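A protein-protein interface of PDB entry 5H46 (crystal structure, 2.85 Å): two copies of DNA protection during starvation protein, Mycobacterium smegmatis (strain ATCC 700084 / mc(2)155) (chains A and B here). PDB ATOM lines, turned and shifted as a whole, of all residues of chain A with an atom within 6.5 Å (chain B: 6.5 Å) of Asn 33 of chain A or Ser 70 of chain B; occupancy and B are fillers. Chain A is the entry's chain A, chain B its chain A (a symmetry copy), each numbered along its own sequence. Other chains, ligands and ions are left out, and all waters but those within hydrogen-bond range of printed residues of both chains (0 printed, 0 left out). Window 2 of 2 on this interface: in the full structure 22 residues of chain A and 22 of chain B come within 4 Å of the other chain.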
ATOM      1  N   LYS A  28      13.876  -1.920 -26.297  1.00  0.00           N
ATOM      2  CA  LYS A  28      15.063  -2.312 -27.069  1.00  0.00           C
ATOM      3  C   LYS A  28      15.576  -3.661 -26.647  1.00  0.00           C
ATOM      4  O   LYS A  28      16.200  -4.338 -27.433  1.00  0.00           O
ATOM      5  CB  LYS A  28      16.136  -1.230 -26.994  1.00  0.00           C
ATOM      6  CG  LYS A  28      17.105  -1.235 -28.155  1.00  0.00           C
ATOM      7  CD  LYS A  28      16.501  -0.680 -29.458  1.00  0.00           C
ATOM      8  CE  LYS A  28      17.502  -0.705 -30.629  1.00  0.00           C
ATOM      9  NZ  LYS A  28      18.366   0.565 -30.763  1.00  0.00           N
ATOM     10  N   HIS A  29      15.304  -4.063 -25.417  1.00  0.00           N
ATOM     11  CA  HIS A  29      15.702  -5.406 -24.934  1.00  0.00           C
ATOM     12  C   HIS A  29      14.828  -6.490 -25.512  1.00  0.00           C
ATOM     13  O   HIS A  29      15.355  -7.473 -26.035  1.00  0.00           O
ATOM     14  CB  HIS A  29      15.715  -5.462 -23.385  1.00  0.00           C
ATOM     15  CG  HIS A  29      15.875  -6.852 -22.832  1.00  0.00           C
ATOM     16  ND1 HIS A  29      14.811  -7.660 -22.491  1.00  0.00           N
ATOM     17  CD2 HIS A  29      16.987  -7.568 -22.573  1.00  0.00           C
ATOM     18  CE1 HIS A  29      15.263  -8.830 -22.088  1.00  0.00           C
ATOM     19  NE2 HIS A  29      16.582  -8.801 -22.148  1.00  0.00           N
ATOM     20  N   VAL A  30      13.517  -6.307 -25.441  1.00  0.00           N
ATOM     21  CA  VAL A  30      12.604  -7.293 -26.040  1.00  0.00           C
ATOM     22  C   VAL A  30      12.855  -7.374 -27.536  1.00  0.00           C
ATOM     23  O   VAL A  30      12.832  -8.473 -28.099  1.00  0.00           O
ATOM     24  CB  VAL A  30      11.105  -7.046 -25.701  1.00  0.00           C
ATOM     25  CG1 VAL A  30      10.930  -6.796 -24.217  1.00  0.00           C
ATOM     26  CG2 VAL A  30      10.575  -5.873 -26.403  1.00  0.00           C
ATOM     27  N   HIS A  31      13.164  -6.218 -28.151  1.00  0.00           N
ATOM     28  CA  HIS A  31      13.438  -6.176 -29.586  1.00  0.00           C
ATOM     29  C   HIS A  31      14.603  -7.099 -29.915  1.00  0.00           C
ATOM     30  O   HIS A  31      14.510  -7.879 -30.839  1.00  0.00           O
ATOM     31  CB  HIS A  31      13.695  -4.731 -30.052  1.00  0.00           C
ATOM     32  CG  HIS A  31      13.948  -4.593 -31.535  1.00  0.00           C
ATOM     33  ND1 HIS A  31      13.034  -4.988 -32.486  1.00  0.00           N
ATOM     34  CD2 HIS A  31      15.026  -4.143 -32.216  1.00  0.00           C
ATOM     35  CE1 HIS A  31      13.538  -4.811 -33.682  1.00  0.00           C
ATOM     36  NE2 HIS A  31      14.755  -4.322 -33.540  1.00  0.00           N
ATOM     37  N   TRP A  32      15.685  -7.021 -29.156  1.00  0.00           N
ATOM     38  CA  TRP A  32      16.881  -7.824 -29.426  1.00  0.00           C
ATOM     39  C   TRP A  32      16.721  -9.323 -29.282  1.00  0.00           C
ATOM     40  O   TRP A  32      17.540 -10.044 -29.834  1.00  0.00           O
ATOM     41  CB  TRP A  32      18.028  -7.399 -28.517  1.00  0.00           C
ATOM     42  CG  TRP A  32      18.624  -6.052 -28.827  1.00  0.00           C
ATOM     43  CD1 TRP A  32      18.841  -5.534 -30.051  1.00  0.00           C
ATOM     44  CD2 TRP A  32      19.145  -5.094 -27.890  1.00  0.00           C
ATOM     45  NE1 TRP A  32      19.415  -4.301 -29.959  1.00  0.00           N
ATOM     46  CE2 TRP A  32      19.627  -4.008 -28.634  1.00  0.00           C
ATOM     47  CE3 TRP A  32      19.221  -5.038 -26.495  1.00  0.00           C
ATOM     48  CZ2 TRP A  32      20.190  -2.880 -28.038  1.00  0.00           C
ATOM     49  CZ3 TRP A  32      19.766  -3.899 -25.911  1.00  0.00           C
ATOM     50  CH2 TRP A  32      20.225  -2.833 -26.697  1.00  0.00           C
ATOM     51  N   ASN A  33      15.708  -9.788 -28.534  1.00  0.00           N
ATOM     52  CA  ASN A  33      15.554 -11.215 -28.258  1.00  0.00           C
ATOM     53  C   ASN A  33      14.524 -11.867 -29.132  1.00  0.00           C
ATOM     54  O   ASN A  33      14.522 -13.100 -29.281  1.00  0.00           O
ATOM     55  CB  ASN A  33      15.194 -11.406 -26.799  1.00  0.00           C
ATOM     56  CG  ASN A  33      16.337 -11.066 -25.875  1.00  0.00           C
ATOM     57  OD1 ASN A  33      17.159 -11.896 -25.599  1.00  0.00           O
ATOM     58  ND2 ASN A  33      16.381  -9.843 -25.400  1.00  0.00           N
ATOM     59  N   VAL A  34      13.638 -11.032 -29.651  1.00  0.00           N
ATOM     60  CA  VAL A  34      12.525 -11.444 -30.468  1.00  0.00           C
ATOM     61  C   VAL A  34      12.769 -11.312 -31.972  1.00  0.00           C
ATOM     62  O   VAL A  34      11.855 -11.440 -32.762  1.00  0.00           O
ATOM     63  CB  VAL A  34      11.264 -10.693 -29.988  1.00  0.00           C
ATOM     64  CG1 VAL A  34      10.599  -9.800 -31.038  1.00  0.00           C
ATOM     65  CG2 VAL A  34      10.303 -11.682 -29.348  1.00  0.00           C
ATOM     66  N   VAL A  35      13.998 -11.121 -32.363  1.00  0.00           N
ATOM     67  CA  VAL A  35      14.359 -10.941 -33.763  1.00  0.00           C
ATOM     68  C   VAL A  35      14.522 -12.234 -34.582  1.00  0.00           C
ATOM     69  O   VAL A  35      15.621 -12.659 -34.851  1.00  0.00           O
ATOM     70  CB  VAL A  35      15.712 -10.258 -33.789  1.00  0.00           C
ATOM     71  CG1 VAL A  35      15.577  -8.848 -33.241  1.00  0.00           C
ATOM     72  CG2 VAL A  35      16.704 -11.037 -32.908  1.00  0.00           C
ATOM     73  N   GLY A  36      13.430 -12.857 -34.989  1.00  0.00           N
ATOM     74  CA  GLY A  36      13.471 -14.129 -35.687  1.00  0.00           C
ATOM     75  C   GLY A  36      12.614 -14.118 -36.931  1.00  0.00           C
ATOM     76  O   GLY A  36      11.787 -13.256 -37.083  1.00  0.00           O
ATOM     77  N   TYR A  87      12.619  -6.740 -16.043  1.00  0.00           N
ATOM     78  CA  TYR A  87      11.998  -7.522 -17.110  1.00  0.00           C
ATOM     79  C   TYR A  87      12.604  -8.913 -17.072  1.00  0.00           C
ATOM     80  O   TYR A  87      13.704  -9.152 -17.580  1.00  0.00           O
ATOM     81  CB  TYR A  87      12.176  -6.877 -18.496  1.00  0.00           C
ATOM     82  CG  TYR A  87      11.518  -7.630 -19.641  1.00  0.00           C
ATOM     83  CD1 TYR A  87      10.213  -7.352 -20.007  1.00  0.00           C
ATOM     84  CD2 TYR A  87      12.214  -8.620 -20.368  1.00  0.00           C
ATOM     85  CE1 TYR A  87       9.621  -8.013 -21.062  1.00  0.00           C
ATOM     86  CE2 TYR A  87      11.617  -9.287 -21.425  1.00  0.00           C
ATOM     87  CZ  TYR A  87      10.339  -8.995 -21.764  1.00  0.00           C
ATOM     88  OH  TYR A  87       9.781  -9.666 -22.833  1.00  0.00           O
ATOM     89  N   ASP A  92      12.243 -18.097 -23.505  1.00  0.00           N
ATOM     90  CA  ASP A  92      12.642 -17.269 -24.635  1.00  0.00           C
ATOM     91  C   ASP A  92      11.800 -17.588 -25.868  1.00  0.00           C
ATOM     92  O   ASP A  92      12.226 -18.274 -26.796  1.00  0.00           O
ATOM     93  CB  ASP A  92      14.150 -17.403 -24.917  1.00  0.00           C
ATOM     94  CG  ASP A  92      14.732 -16.212 -25.711  1.00  0.00           C
ATOM     95  OD1 ASP A  92      14.066 -15.170 -25.791  1.00  0.00           O
ATOM     96  OD2 ASP A  92      15.859 -16.328 -26.241  1.00  0.00           O
ATOM     97  N   THR A  93      10.585 -17.066 -25.867  1.00  0.00           N
ATOM     98  CA  THR A  93       9.722 -17.173 -27.012  1.00  0.00           C
ATOM     99  C   THR A  93       9.048 -15.839 -27.284  1.00  0.00           C
ATOM    100  O   THR A  93       9.122 -14.897 -26.496  1.00  0.00           O
ATOM    101  CB  THR A  93       8.681 -18.297 -26.851  1.00  0.00           C
ATOM    102  OG1 THR A  93       7.924 -18.395 -28.072  1.00  0.00           O
ATOM    103  CG2 THR A  93       7.732 -18.016 -25.724  1.00  0.00           C
ATOM    104  N   HIS A  97       7.669 -13.106 -24.208  1.00  0.00           N
ATOM    105  CA  HIS A  97       8.140 -11.731 -24.235  1.00  0.00           C
ATOM    106  C   HIS A  97       6.989 -10.724 -24.400  1.00  0.00           C
ATOM    107  O   HIS A  97       6.948  -9.704 -23.724  1.00  0.00           O
ATOM    108  CB  HIS A  97       9.147 -11.568 -25.337  1.00  0.00           C
ATOM    109  CG  HIS A  97      10.516 -12.005 -24.977  1.00  0.00           C
ATOM    110  ND1 HIS A  97      11.350 -11.225 -24.201  1.00  0.00           N
ATOM    111  CD2 HIS A  97      11.213 -13.122 -25.291  1.00  0.00           C
ATOM    112  CE1 HIS A  97      12.509 -11.855 -24.053  1.00  0.00           C
ATOM    113  NE2 HIS A  97      12.459 -12.998 -24.730  1.00  0.00           N
ATOM    114  N   GLN B  14      28.244  -8.891 -23.011  1.00  0.00           N
ATOM    115  CA  GLN B  14      27.099  -8.493 -22.215  1.00  0.00           C
ATOM    116  C   GLN B  14      27.457  -7.310 -21.310  1.00  0.00           C
ATOM    117  O   GLN B  14      26.622  -6.447 -21.019  1.00  0.00           O
ATOM    118  CB  GLN B  14      26.601  -9.679 -21.431  1.00  0.00           C
ATOM    119  CG  GLN B  14      25.471  -9.363 -20.457  1.00  0.00           C
ATOM    120  CD  GLN B  14      24.346  -8.624 -21.129  1.00  0.00           C
ATOM    121  OE1 GLN B  14      23.668  -9.181 -22.016  1.00  0.00           O
ATOM    122  NE2 GLN B  14      24.131  -7.362 -20.703  1.00  0.00           N
ATOM    123  N   LEU B  17      27.752  -4.350 -23.863  1.00  0.00           N
ATOM    124  CA  LEU B  17      26.393  -3.936 -24.112  1.00  0.00           C
ATOM    125  C   LEU B  17      25.883  -2.989 -23.043  1.00  0.00           C
ATOM    126  O   LEU B  17      25.252  -1.957 -23.373  1.00  0.00           O
ATOM    127  CB  LEU B  17      25.483  -5.148 -24.213  1.00  0.00           C
ATOM    128  CG  LEU B  17      24.219  -5.086 -25.098  1.00  0.00           C
ATOM    129  CD1 LEU B  17      23.619  -6.490 -25.157  1.00  0.00           C
ATOM    130  CD2 LEU B  17      23.174  -4.125 -24.605  1.00  0.00           C
ATOM    131  N   ALA B  61      24.721  -6.433 -29.145  1.00  0.00           N
ATOM    132  CA  ALA B  61      23.534  -7.249 -28.947  1.00  0.00           C
ATOM    133  C   ALA B  61      23.400  -8.311 -30.029  1.00  0.00           C
ATOM    134  O   ALA B  61      23.264  -9.489 -29.749  1.00  0.00           O
ATOM    135  CB  ALA B  61      22.299  -6.379 -28.923  1.00  0.00           C
ATOM    136  N   ILE B  64      26.023 -11.031 -29.578  1.00  0.00           N
ATOM    137  CA  ILE B  64      25.654 -11.933 -28.506  1.00  0.00           C
ATOM    138  C   ILE B  64      24.651 -12.956 -29.030  1.00  0.00           C
ATOM    139  O   ILE B  64      24.832 -14.169 -28.848  1.00  0.00           O
ATOM    140  CB  ILE B  64      25.073 -11.140 -27.303  1.00  0.00           C
ATOM    141  CG1 ILE B  64      26.203 -10.465 -26.538  1.00  0.00           C
ATOM    142  CG2 ILE B  64      24.266 -11.985 -26.369  1.00  0.00           C
ATOM    143  CD1 ILE B  64      25.714  -9.412 -25.558  1.00  0.00           C
ATOM    144  N   ALA B  65      23.593 -12.485 -29.682  1.00  0.00           N
ATOM    145  CA  ALA B  65      22.568 -13.389 -30.217  1.00  0.00           C
ATOM    146  C   ALA B  65      23.135 -14.362 -31.231  1.00  0.00           C
ATOM    147  O   ALA B  65      22.709 -15.503 -31.282  1.00  0.00           O
ATOM    148  CB  ALA B  65      21.421 -12.594 -30.814  1.00  0.00           C
ATOM    149  N   GLY B  68      24.617 -17.359 -29.551  1.00  0.00           N
ATOM    150  CA  GLY B  68      23.666 -18.291 -28.976  1.00  0.00           C
ATOM    151  C   GLY B  68      22.973 -17.812 -27.716  1.00  0.00           C
ATOM    152  O   GLY B  68      21.914 -18.325 -27.341  1.00  0.00           O
ATOM    153  N   LYS B  69      23.553 -16.819 -27.054  1.00  0.00           N
ATOM    154  CA  LYS B  69      22.982 -16.289 -25.828  1.00  0.00           C
ATOM    155  C   LYS B  69      21.946 -15.197 -26.135  1.00  0.00           C
ATOM    156  O   LYS B  69      21.677 -14.882 -27.312  1.00  0.00           O
ATOM    157  CB  LYS B  69      24.105 -15.785 -24.938  1.00  0.00           C
ATOM    158  CG  LYS B  69      25.290 -16.745 -24.800  1.00  0.00           C
ATOM    159  CD  LYS B  69      24.913 -18.192 -24.463  1.00  0.00           C
ATOM    160  CE  LYS B  69      25.959 -18.827 -23.521  1.00  0.00           C
ATOM    161  NZ  LYS B  69      25.768 -20.287 -23.433  1.00  0.00           N
ATOM    162  N   SER B  70      21.319 -14.649 -25.089  1.00  0.00           N
ATOM    163  CA  SER B  70      20.323 -13.606 -25.263  1.00  0.00           C
ATOM    164  C   SER B  70      20.837 -12.317 -24.630  1.00  0.00           C
ATOM    165  O   SER B  70      21.329 -12.337 -23.507  1.00  0.00           O
ATOM    166  CB  SER B  70      18.971 -14.005 -24.695  1.00  0.00           C
ATOM    167  OG  SER B  70      18.967 -13.928 -23.331  1.00  0.00           O
ATOM    168  N   PRO B  71      20.731 -11.180 -25.357  1.00  0.00           N
ATOM    169  CA  PRO B  71      21.238  -9.926 -24.840  1.00  0.00           C
ATOM    170  C   PRO B  71      20.365  -9.310 -23.769  1.00  0.00           C
ATOM    171  O   PRO B  71      19.154  -9.431 -23.798  1.00  0.00           O
ATOM    172  CB  PRO B  71      21.315  -9.045 -26.082  1.00  0.00           C
ATOM    173  CG  PRO B  71      21.129  -9.963 -27.237  1.00  0.00           C
ATOM    174  CD  PRO B  71      20.259 -11.040 -26.736  1.00  0.00           C
ATOM    175  N   LYS B  72      20.999  -8.659 -22.825  1.00  0.00           N
ATOM    176  CA  LYS B  72      20.265  -8.041 -21.760  1.00  0.00           C
ATOM    177  C   LYS B  72      20.640  -6.580 -21.712  1.00  0.00           C
ATOM    178  O   LYS B  72      21.803  -6.196 -21.527  1.00  0.00           O
ATOM    179  CB  LYS B  72      20.518  -8.763 -20.451  1.00  0.00           C
ATOM    180  CG  LYS B  72      20.347 -10.287 -20.523  1.00  0.00           C
ATOM    181  CD  LYS B  72      18.949 -10.755 -20.143  1.00  0.00           C
ATOM    182  CE  LYS B  72      18.348 -11.721 -21.164  1.00  0.00           C
ATOM    183  NZ  LYS B  72      16.880 -12.002 -20.917  1.00  0.00           N
ATOM    184  N   GLY B  73      19.666  -5.720 -21.910  1.00  0.00           N
ATOM    185  CA  GLY B  73      19.953  -4.291 -21.779  1.00  0.00           C
ATOM    186  C   GLY B  73      18.943  -3.596 -20.935  1.00  0.00           C
ATOM    187  O   GLY B  73      18.773  -2.395 -21.014  1.00  0.00           O
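The backbone carbonyl oxygen (O) of Pro 71 of chain B sits close to a ring nitrogen (NE2) of His 29 of chain A. NZ of Lys 72 of chain B lies within hydrogen-bond range of NE2 of His 29 of chain A (3.4 Å). The side-chain amide nitrogen (ND2) of Asn 33 of chain A is in hydrogen-bond range of the backbone carbonyl oxygen (O) of Pro 71 of chain B.
The side-chain amide nitrogen of Asn 33 of chain A is in hydrogen-bond range of the backbone carbonyl oxygen of His 29 of chain A. NE2 of Gln 14 of chain B lies within hydrogen-bond range of O of Lys 72 of chain B.
Among the printed residues, merely in contact across the chains: His 29 of chain A with Gly 73 of chain B, Trp 32 of chain A with Leu 17 of chain B, Trp 32 of chain A with Ala 61 of chain B and Asn 33 of chain A with Ser 70 of chain B.
Of the printed residues of chain B, Asn 33 of chain A touches Ser 70 (2.9 Å) and Pro 71 (3.2 Å). Ser 70 of chain B touches one residue of chain A. Printed residues of chain B within 4 Å of His 29 of chain A: Pro 71 (3.1 Å), Lys 72 (3.4 Å) and Gly 73 (3.3 Å). Of the printed residues of chain A, Leu 17 of chain B touches Trp 32 (3.7 Å).
Hydrophobic or aromatic side chains of chain B within 4 Å of the printed part of chain A: Leu 17, Ala 61 and Pro 71.
No position is printed for both chains. Of the 7 pairs that touch across the chains among the printed residues, none has its exchanged pair printed and touching as well.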
